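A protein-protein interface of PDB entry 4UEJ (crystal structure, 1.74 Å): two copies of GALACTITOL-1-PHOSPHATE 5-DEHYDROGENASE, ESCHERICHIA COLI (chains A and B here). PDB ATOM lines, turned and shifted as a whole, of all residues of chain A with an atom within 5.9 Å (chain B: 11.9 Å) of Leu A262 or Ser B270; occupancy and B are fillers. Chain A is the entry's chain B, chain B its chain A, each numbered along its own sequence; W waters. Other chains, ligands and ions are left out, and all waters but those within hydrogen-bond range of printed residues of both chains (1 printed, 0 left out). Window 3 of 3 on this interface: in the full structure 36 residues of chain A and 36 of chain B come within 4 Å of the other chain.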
ATOM      1  N   GLU A 235      -8.920 -25.143  37.250  1.00  0.00           N
ATOM      2  CA  GLU A 235      -8.961 -23.696  37.137  1.00  0.00           C
ATOM      3  C   GLU A 235     -10.356 -23.234  37.528  1.00  0.00           C
ATOM      4  O   GLU A 235     -11.286 -23.405  36.750  1.00  0.00           O
ATOM      5  CB  GLU A 235      -8.625 -23.262  35.697  1.00  0.00           C
ATOM      6  CG  GLU A 235      -8.084 -21.849  35.600  1.00  0.00           C
ATOM      7  CD  GLU A 235      -9.001 -20.834  36.266  1.00  0.00           C
ATOM      8  OE1 GLU A 235     -10.127 -20.599  35.759  1.00  0.00           O
ATOM      9  OE2 GLU A 235      -8.618 -20.328  37.339  1.00  0.00           O
ATOM     10  N   GLY A 238     -11.502 -18.444  36.814  1.00  0.00           N
ATOM     11  CA  GLY A 238     -12.116 -17.874  35.626  1.00  0.00           C
ATOM     12  C   GLY A 238     -11.620 -16.483  35.272  1.00  0.00           C
ATOM     13  O   GLY A 238     -12.411 -15.602  34.920  1.00  0.00           O
ATOM     14  N   VAL A 239     -10.315 -16.263  35.393  1.00  0.00           N
ATOM     15  CA  VAL A 239      -9.719 -15.054  34.841  1.00  0.00           C
ATOM     16  C   VAL A 239      -8.553 -15.468  33.942  1.00  0.00           C
ATOM     17  O   VAL A 239      -7.990 -16.542  34.125  1.00  0.00           O
ATOM     18  CB  VAL A 239      -9.247 -14.073  35.933  1.00  0.00           C
ATOM     19  CG1 VAL A 239     -10.433 -13.586  36.764  1.00  0.00           C
ATOM     20  CG2 VAL A 239      -8.193 -14.713  36.791  1.00  0.00           C
ATOM     21  N   PRO A 240      -8.218 -14.638  32.942  1.00  0.00           N
ATOM     22  CA  PRO A 240      -7.174 -15.039  31.991  1.00  0.00           C
ATOM     23  C   PRO A 240      -5.851 -15.389  32.661  1.00  0.00           C
ATOM     24  O   PRO A 240      -5.166 -16.311  32.211  1.00  0.00           O
ATOM     25  CB  PRO A 240      -7.019 -13.805  31.092  1.00  0.00           C
ATOM     26  CG  PRO A 240      -7.676 -12.700  31.816  1.00  0.00           C
ATOM     27  CD  PRO A 240      -8.770 -13.314  32.611  1.00  0.00           C
ATOM     28  N   VAL A 243      -5.760 -19.081  33.967  1.00  0.00           N
ATOM     29  CA  VAL A 243      -5.667 -20.079  32.905  1.00  0.00           C
ATOM     30  C   VAL A 243      -4.214 -20.142  32.435  1.00  0.00           C
ATOM     31  O   VAL A 243      -3.635 -21.226  32.300  1.00  0.00           O
ATOM     32  CB  VAL A 243      -6.589 -19.772  31.697  1.00  0.00           C
ATOM     33  CG1 VAL A 243      -6.447 -20.858  30.625  1.00  0.00           C
ATOM     34  CG2 VAL A 243      -8.031 -19.660  32.130  1.00  0.00           C
ATOM     35  N   GLY A 260     -13.822 -22.375  35.562  1.00  0.00           N
ATOM     36  CA  GLY A 260     -14.144 -20.961  35.594  1.00  0.00           C
ATOM     37  C   GLY A 260     -14.435 -20.367  34.225  1.00  0.00           C
ATOM     38  O   GLY A 260     -13.642 -20.478  33.297  1.00  0.00           O
ATOM     39  N   THR A 261     -15.579 -19.711  34.093  1.00  0.00           N
ATOM     40  CA  THR A 261     -15.892 -19.066  32.827  1.00  0.00           C
ATOM     41  C   THR A 261     -15.187 -17.718  32.773  1.00  0.00           C
ATOM     42  O   THR A 261     -15.182 -16.966  33.753  1.00  0.00           O
ATOM     43  CB  THR A 261     -17.407 -18.863  32.638  1.00  0.00           C
ATOM     44  OG1 THR A 261     -17.813 -17.669  33.311  1.00  0.00           O
ATOM     45  CG2 THR A 261     -18.175 -20.047  33.198  1.00  0.00           C
ATOM     46  N   LEU A 262     -14.575 -17.412  31.640  1.00  0.00           N
ATOM     47  CA  LEU A 262     -13.926 -16.123  31.475  1.00  0.00           C
ATOM     48  C   LEU A 262     -14.944 -15.078  31.067  1.00  0.00           C
ATOM     49  O   LEU A 262     -15.866 -15.354  30.300  1.00  0.00           O
ATOM     50  CB  LEU A 262     -12.807 -16.202  30.440  1.00  0.00           C
ATOM     51  CG  LEU A 262     -11.385 -16.423  30.949  1.00  0.00           C
ATOM     52  CD1 LEU A 262     -11.312 -17.516  31.996  1.00  0.00           C
ATOM     53  CD2 LEU A 262     -10.516 -16.769  29.765  1.00  0.00           C
ATOM     54  N   HIS A 263     -14.782 -13.875  31.602  1.00  0.00           N
ATOM     55  CA  HIS A 263     -15.589 -12.745  31.185  1.00  0.00           C
ATOM     56  C   HIS A 263     -14.668 -11.712  30.566  1.00  0.00           C
ATOM     57  O   HIS A 263     -15.071 -10.593  30.254  1.00  0.00           O
ATOM     58  CB  HIS A 263     -16.377 -12.184  32.368  1.00  0.00           C
ATOM     59  CG  HIS A 263     -17.374 -13.155  32.915  1.00  0.00           C
ATOM     60  ND1 HIS A 263     -18.707 -13.131  32.564  1.00  0.00           N
ATOM     61  CD2 HIS A 263     -17.223 -14.211  33.750  1.00  0.00           C
ATOM     62  CE1 HIS A 263     -19.337 -14.118  33.176  1.00  0.00           C
ATOM     63  NE2 HIS A 263     -18.460 -14.787  33.903  1.00  0.00           N
ATOM     64  N   GLN A 264     -13.421 -12.125  30.385  1.00  0.00           N
ATOM     65  CA  GLN A 264     -12.413 -11.331  29.702  1.00  0.00           C
ATOM     66  C   GLN A 264     -11.753 -12.231  28.657  1.00  0.00           C
ATOM     67  O   GLN A 264     -11.717 -13.444  28.838  1.00  0.00           O
ATOM     68  CB  GLN A 264     -11.374 -10.788  30.685  1.00  0.00           C
ATOM     69  CG  GLN A 264     -10.377  -9.820  30.062  1.00  0.00           C
ATOM     70  CD  GLN A 264      -9.409  -9.222  31.075  1.00  0.00           C
ATOM     71  OE1 GLN A 264      -9.444  -9.551  32.267  1.00  0.00           O
ATOM     72  NE2 GLN A 264      -8.536  -8.335  30.599  1.00  0.00           N
ATOM     73  N   ASP A 265     -11.247 -11.647  27.576  1.00  0.00           N
ATOM     74  CA  ASP A 265     -10.547 -12.434  26.555  1.00  0.00           C
ATOM     75  C   ASP A 265      -9.263 -13.049  27.118  1.00  0.00           C
ATOM     76  O   ASP A 265      -8.727 -12.584  28.125  1.00  0.00           O
ATOM     77  CB  ASP A 265     -10.226 -11.573  25.329  1.00  0.00           C
ATOM     78  CG  ASP A 265     -11.463 -11.221  24.516  1.00  0.00           C
ATOM     79  OD1 ASP A 265     -12.588 -11.582  24.943  1.00  0.00           O
ATOM     80  OD2 ASP A 265     -11.307 -10.586  23.446  1.00  0.00           O
ATOM     81  N   LEU A 266      -8.795 -14.114  26.473  1.00  0.00           N
ATOM     82  CA  LEU A 266      -7.566 -14.806  26.863  1.00  0.00           C
ATOM     83  C   LEU A 266      -6.487 -14.634  25.810  1.00  0.00           C
ATOM     84  O   LEU A 266      -6.637 -15.076  24.684  1.00  0.00           O
ATOM     85  CB  LEU A 266      -7.820 -16.302  27.071  1.00  0.00           C
ATOM     86  CG  LEU A 266      -6.572 -17.133  27.372  1.00  0.00           C
ATOM     87  CD1 LEU A 266      -6.001 -16.749  28.741  1.00  0.00           C
ATOM     88  CD2 LEU A 266      -6.899 -18.622  27.317  1.00  0.00           C
ATOM     89  N   GLU B 244      -8.318 -21.349  16.725  1.00  0.00           N
ATOM     90  CA  GLU B 244      -9.618 -20.721  16.938  1.00  0.00           C
ATOM     91  C   GLU B 244     -10.718 -21.420  16.145  1.00  0.00           C
ATOM     92  O   GLU B 244     -11.801 -21.689  16.674  1.00  0.00           O
ATOM     93  CB  GLU B 244      -9.564 -19.240  16.557  1.00  0.00           C
ATOM     94  CG  GLU B 244     -10.879 -18.503  16.679  1.00  0.00           C
ATOM     95  CD  GLU B 244     -10.767 -17.049  16.239  1.00  0.00           C
ATOM     96  OE1 GLU B 244     -10.167 -16.791  15.176  1.00  0.00           O
ATOM     97  OE2 GLU B 244     -11.274 -16.165  16.957  1.00  0.00           O
ATOM     98  N   VAL B 247     -11.925 -24.755  17.666  1.00  0.00           N
ATOM     99  CA  VAL B 247     -12.821 -24.592  18.799  1.00  0.00           C
ATOM    100  C   VAL B 247     -14.200 -24.160  18.328  1.00  0.00           C
ATOM    101  O   VAL B 247     -15.217 -24.658  18.811  1.00  0.00           O
ATOM    102  CB  VAL B 247     -12.268 -23.567  19.805  1.00  0.00           C
ATOM    103  CG1 VAL B 247     -13.315 -23.259  20.889  1.00  0.00           C
ATOM    104  CG2 VAL B 247     -10.990 -24.112  20.428  1.00  0.00           C
ATOM    105  N   GLU B 248     -14.238 -23.244  17.364  1.00  0.00           N
ATOM    106  CA  GLU B 248     -15.516 -22.736  16.874  1.00  0.00           C
ATOM    107  C   GLU B 248     -16.354 -23.790  16.143  1.00  0.00           C
ATOM    108  O   GLU B 248     -17.584 -23.775  16.238  1.00  0.00           O
ATOM    109  CB  GLU B 248     -15.294 -21.521  15.962  1.00  0.00           C
ATOM    110  CG  GLU B 248     -14.849 -20.282  16.740  1.00  0.00           C
ATOM    111  CD  GLU B 248     -15.944 -19.740  17.653  1.00  0.00           C
ATOM    112  OE1 GLU B 248     -17.137 -19.961  17.355  1.00  0.00           O
ATOM    113  OE2 GLU B 248     -15.620 -19.089  18.665  1.00  0.00           O
ATOM    114  N   LEU B 266      -1.845 -16.434  20.588  1.00  0.00           N
ATOM    115  CA  LEU B 266      -3.222 -16.839  20.386  1.00  0.00           C
ATOM    116  C   LEU B 266      -4.120 -15.951  21.223  1.00  0.00           C
ATOM    117  O   LEU B 266      -4.028 -15.972  22.441  1.00  0.00           O
ATOM    118  CB  LEU B 266      -3.412 -18.310  20.770  1.00  0.00           C
ATOM    119  CG  LEU B 266      -4.825 -18.884  20.669  1.00  0.00           C
ATOM    120  CD1 LEU B 266      -5.322 -18.831  19.221  1.00  0.00           C
ATOM    121  CD2 LEU B 266      -4.854 -20.312  21.190  1.00  0.00           C
ATOM    122  N   HIS B 267      -4.977 -15.165  20.582  1.00  0.00           N
ATOM    123  CA  HIS B 267      -5.980 -14.396  21.310  1.00  0.00           C
ATOM    124  C   HIS B 267      -7.329 -15.068  21.125  1.00  0.00           C
ATOM    125  O   HIS B 267      -7.842 -15.139  20.011  1.00  0.00           O
ATOM    126  CB  HIS B 267      -6.032 -12.936  20.832  1.00  0.00           C
ATOM    127  CG  HIS B 267      -7.018 -12.088  21.581  1.00  0.00           C
ATOM    128  ND1 HIS B 267      -6.639 -11.014  22.357  1.00  0.00           N
ATOM    129  CD2 HIS B 267      -8.369 -12.158  21.672  1.00  0.00           C
ATOM    130  CE1 HIS B 267      -7.713 -10.462  22.896  1.00  0.00           C
ATOM    131  NE2 HIS B 267      -8.776 -11.136  22.493  1.00  0.00           N
ATOM    132  N   LEU B 268      -7.904 -15.576  22.207  1.00  0.00           N
ATOM    133  CA  LEU B 268      -9.247 -16.131  22.123  1.00  0.00           C
ATOM    134  C   LEU B 268     -10.215 -15.187  22.806  1.00  0.00           C
ATOM    135  O   LEU B 268      -9.969 -14.743  23.920  1.00  0.00           O
ATOM    136  CB  LEU B 268      -9.322 -17.518  22.764  1.00  0.00           C
ATOM    137  CG  LEU B 268      -8.510 -18.661  22.154  1.00  0.00           C
ATOM    138  CD1 LEU B 268      -8.817 -19.949  22.898  1.00  0.00           C
ATOM    139  CD2 LEU B 268      -8.803 -18.817  20.673  1.00  0.00           C
ATOM    140  N   THR B 269     -11.314 -14.871  22.138  1.00  0.00           N
ATOM    141  CA  THR B 269     -12.376 -14.130  22.791  1.00  0.00           C
ATOM    142  C   THR B 269     -12.915 -14.955  23.952  1.00  0.00           C
ATOM    143  O   THR B 269     -12.765 -16.179  23.975  1.00  0.00           O
ATOM    144  CB  THR B 269     -13.510 -13.816  21.828  1.00  0.00           C
ATOM    145  OG1 THR B 269     -14.121 -15.048  21.433  1.00  0.00           O
ATOM    146  CG2 THR B 269     -12.973 -13.105  20.600  1.00  0.00           C
ATOM    147  N   SER B 270     -13.551 -14.295  24.912  1.00  0.00           N
ATOM    148  CA  SER B 270     -14.154 -15.019  26.020  1.00  0.00           C
ATOM    149  C   SER B 270     -15.213 -15.979  25.487  1.00  0.00           C
ATOM    150  O   SER B 270     -15.430 -17.056  26.049  1.00  0.00           O
ATOM    151  CB  SER B 270     -14.760 -14.051  27.042  1.00  0.00           C
ATOM    152  OG  SER B 270     -15.674 -13.171  26.423  1.00  0.00           O
ATOM    153  N   ALA B 271     -15.852 -15.582  24.389  1.00  0.00           N
ATOM    154  CA  ALA B 271     -16.849 -16.418  23.743  1.00  0.00           C
ATOM    155  C   ALA B 271     -16.221 -17.721  23.264  1.00  0.00           C
ATOM    156  O   ALA B 271     -16.728 -18.803  23.565  1.00  0.00           O
ATOM    157  CB  ALA B 271     -17.497 -15.677  22.581  1.00  0.00           C
ATOM    158  N   THR B 272     -15.117 -17.617  22.528  1.00  0.00           N
ATOM    159  CA  THR B 272     -14.451 -18.806  22.001  1.00  0.00           C
ATOM    160  C   THR B 272     -13.902 -19.655  23.135  1.00  0.00           C
ATOM    161  O   THR B 272     -14.057 -20.874  23.129  1.00  0.00           O
ATOM    162  CB  THR B 272     -13.300 -18.447  21.032  1.00  0.00           C
ATOM    163  OG1 THR B 272     -13.814 -17.684  19.935  1.00  0.00           O
ATOM    164  CG2 THR B 272     -12.624 -19.711  20.504  1.00  0.00           C
ATOM    165  N   PHE B 273     -13.263 -19.013  24.113  1.00  0.00           N
ATOM    166  CA  PHE B 273     -12.763 -19.757  25.263  1.00  0.00           C
ATOM    167  C   PHE B 273     -13.918 -20.486  25.943  1.00  0.00           C
ATOM    168  O   PHE B 273     -13.799 -21.653  26.305  1.00  0.00           O
ATOM    169  CB  PHE B 273     -12.064 -18.843  26.269  1.00  0.00           C
ATOM    170  CG  PHE B 273     -11.655 -19.552  27.531  1.00  0.00           C
ATOM    171  CD1 PHE B 273     -10.453 -20.228  27.596  1.00  0.00           C
ATOM    172  CD2 PHE B 273     -12.484 -19.552  28.649  1.00  0.00           C
ATOM    173  CE1 PHE B 273     -10.075 -20.882  28.761  1.00  0.00           C
ATOM    174  CE2 PHE B 273     -12.117 -20.213  29.806  1.00  0.00           C
ATOM    175  CZ  PHE B 273     -10.912 -20.878  29.859  1.00  0.00           C
ATOM    176  N   GLY B 274     -15.031 -19.782  26.098  1.00  0.00           N
ATOM    177  CA  GLY B 274     -16.221 -20.330  26.722  1.00  0.00           C
ATOM    178  C   GLY B 274     -16.742 -21.583  26.041  1.00  0.00           C
ATOM    179  O   GLY B 274     -17.311 -22.454  26.694  1.00  0.00           O
ATOM    180  N   LYS B 275     -16.549 -21.676  24.728  1.00  0.00           N
ATOM    181  CA  LYS B 275     -16.994 -22.848  23.987  1.00  0.00           C
ATOM    182  C   LYS B 275     -16.184 -24.076  24.357  1.00  0.00           C
ATOM    183  O   LYS B 275     -16.694 -25.192  24.287  1.00  0.00           O
ATOM    184  CB  LYS B 275     -16.918 -22.605  22.476  1.00  0.00           C
ATOM    185  CG  LYS B 275     -17.960 -21.610  22.000  1.00  0.00           C
ATOM    186  CD  LYS B 275     -17.985 -21.483  20.476  1.00  0.00           C
ATOM    187  CE  LYS B 275     -19.124 -20.561  20.056  1.00  0.00           C
ATOM    188  NZ  LYS B 275     -19.349 -20.532  18.565  1.00  0.00           N
ATOM    189  N   ILE B 276     -14.921 -23.893  24.741  1.00  0.00           N
ATOM    190  CA  ILE B 276     -14.159 -25.050  25.203  1.00  0.00           C
ATOM    191  C   ILE B 276     -14.871 -25.670  26.396  1.00  0.00           C
ATOM    192  O   ILE B 276     -15.005 -26.893  26.486  1.00  0.00           O
ATOM    193  CB  ILE B 276     -12.722 -24.678  25.599  1.00  0.00           C
ATOM    194  CG1 ILE B 276     -11.983 -24.099  24.403  1.00  0.00           C
ATOM    195  CG2 ILE B 276     -12.006 -25.882  26.194  1.00  0.00           C
ATOM    196  CD1 ILE B 276     -10.641 -23.511  24.758  1.00  0.00           C
ATOM    197  N   LEU B 277     -15.335 -24.814  27.311  1.00  0.00           N
ATOM    198  CA  LEU B 277     -16.104 -25.276  28.463  1.00  0.00           C
ATOM    199  C   LEU B 277     -17.484 -25.777  28.061  1.00  0.00           C
ATOM    200  O   LEU B 277     -17.854 -26.905  28.376  1.00  0.00           O
ATOM    201  CB  LEU B 277     -16.251 -24.165  29.511  1.00  0.00           C
ATOM    202  CG  LEU B 277     -15.014 -23.958  30.394  1.00  0.00           C
ATOM    203  CD1 LEU B 277     -13.889 -23.308  29.614  1.00  0.00           C
ATOM    204  CD2 LEU B 277     -15.380 -23.123  31.622  1.00  0.00           C
ATOM    205  N   ARG B 278     -18.232 -24.941  27.355  1.00  0.00           N
ATOM    206  CA  ARG B 278     -19.624 -25.263  27.045  1.00  0.00           C
ATOM    207  C   ARG B 278     -19.794 -26.529  26.215  1.00  0.00           C
ATOM    208  O   ARG B 278     -20.751 -27.277  26.421  1.00  0.00           O
ATOM    209  CB  ARG B 278     -20.283 -24.087  26.343  1.00  0.00           C
ATOM    210  CG  ARG B 278     -20.611 -22.938  27.287  1.00  0.00           C
ATOM    211  CD  ARG B 278     -21.269 -21.813  26.511  1.00  0.00           C
ATOM    212  NE  ARG B 278     -22.005 -20.907  27.385  1.00  0.00           N
ATOM    213  CZ  ARG B 278     -21.449 -19.890  28.021  1.00  0.00           C
ATOM    214  NH1 ARG B 278     -20.152 -19.663  27.879  1.00  0.00           N
ATOM    215  NH2 ARG B 278     -22.185 -19.103  28.797  1.00  0.00           N
ATOM    216  N   LYS B 279     -18.881 -26.762  25.274  1.00  0.00           N
ATOM    217  CA  LYS B 279     -18.908 -27.981  24.481  1.00  0.00           C
ATOM    218  C   LYS B 279     -18.239 -29.139  25.198  1.00  0.00           C
ATOM    219  O   LYS B 279     -18.270 -30.268  24.722  1.00  0.00           O
ATOM    220  CB  LYS B 279     -18.228 -27.767  23.119  1.00  0.00           C
ATOM    221  CG  LYS B 279     -18.831 -26.632  22.304  1.00  0.00           C
ATOM    222  CD  LYS B 279     -18.043 -26.447  21.013  1.00  0.00           C
ATOM    223  CE  LYS B 279     -18.621 -25.308  20.191  1.00  0.00           C
ATOM    224  NZ  LYS B 279     -18.005 -25.247  18.834  1.00  0.00           N
ATOM    225  N   LEU B 281     -15.052 -29.725  25.469  1.00  0.00           N
ATOM    226  CA  LEU B 281     -14.009 -30.253  24.608  1.00  0.00           C
ATOM    227  C   LEU B 281     -12.903 -30.870  25.453  1.00  0.00           C
ATOM    228  O   LEU B 281     -12.737 -30.542  26.634  1.00  0.00           O
ATOM    229  CB  LEU B 281     -13.428 -29.154  23.730  1.00  0.00           C
ATOM    230  CG  LEU B 281     -14.435 -28.381  22.888  1.00  0.00           C
ATOM    231  CD1 LEU B 281     -13.704 -27.390  22.011  1.00  0.00           C
ATOM    232  CD2 LEU B 281     -15.263 -29.362  22.051  1.00  0.00           C
HETATM  233  O   HOH W   1     -15.849 -17.623  28.666  1.00  0.00           O
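Leu A266 touches its own counterpart, Leu B266. Of the 14 pairs that touch across the chains among the printed residues, 1 has its exchanged pair printed and touching as well.
The side-chain hydroxyl of Thr B269 lies close to the backbone NH of Ala B271 (3.5 Å). The side-chain hydroxyl (OG1) of Thr B269 lies within hydrogen-bond range of the backbone NH (N) of Thr B272 (3.0 Å). The backbone NH of Gly A260 sits at hydrogen-bond distance from the backbone carbonyl oxygen of Glu A235, 3.0 Å away.
No residue of chain B comes within 4 Å of Gly A238. No residue of chain B comes within 4 Å of Val A239. No residue of chain B comes within 4 Å of Pro A240. Of the printed residues of chain B, Val A243 touches Phe B273 (3.9 Å). Leu A262 touches just these residues of chain B: Ser B270 and Phe B273. No residue of chain B comes within 4 Å of His A263. Printed residues of chain B within 4 Å of Gln A264: Ser B270. Leu A266 touches just these residues of chain B: Leu B266 (3.6 Å), His B267 (3.5 Å), Leu B268 (2.8 Å) and Phe B273 (3.9 Å). Glu B244 touches none of the printed residues of chain A. Of the printed residues of chain A, Leu B268 touches Asp A265 and Leu A266. Of the printed residues of chain A, Ser B270 touches Leu A262, Gln A264 and Asp A265. Arg B278 touches none of the printed residues of chain A. The nearest residue of chain A that does not touch Ser B270 is His A263 (4.2 Å).
Of the 18 printed residues of chain B, 7 touch a printed residue of chain A. Hydrophobic or aromatic side chains of chain B that line the printed part of chain A: His B267, Phe B273 and Leu B277. Printed residues of chain A that touch a printed residue of chain B: Val A243, Gly A260, Leu A262, Gln A264, Asp A265 and Leu A266. Hydrophobic or aromatic side chains of chain A that line the printed part of chain B: Val A243, Leu A262 and Leu A266. Along chain A the printed residues that touch a printed residue of chain B span positions 243 to 266. Among the printed residues, 14 pairs touch across the chains. Among the printed residues, no Asp or Glu carboxylate lies within 4 Å of a Lys or Arg side-chain nitrogen of the other chain.
A ring nitrogen (NE2) of His B267 lies within hydrogen-bond range of the side-chain carboxylate (OD2) of Asp A265, 2.8 Å away. N of Leu B268 sits at hydrogen-bond distance from O of Leu A266 (2.8 Å). The backbone NH (N) of Ser B270 sits at hydrogen-bond distance from the side-chain carboxylate (OD1) of Asp A265.
Water W1 lies within hydrogen-bond range of O of Ser B270, O of Leu A262 and N of Gly B274.
Phe B273 touches Val A243 (CZ to CG2, 3.9 Å). CE2 of Phe B273 touches O of Gly A260 (3.8 Å). Gly A260 touches Leu B277 (O to CD2, 3.6 Å). Ser B270 touches Leu A262 (CB to O, 3.7 Å). Leu A262 touches Phe B273 (CD1 to CE2, 3.6 Å). Asp A265 touches Leu B268. Thr B269 touches Asp A265. O of Leu A266 touches O of Leu B266, at 3.6 Å. Leu A266 touches His B267 (O to CA, 3.5 Å). Phe B273 touches Leu A266.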
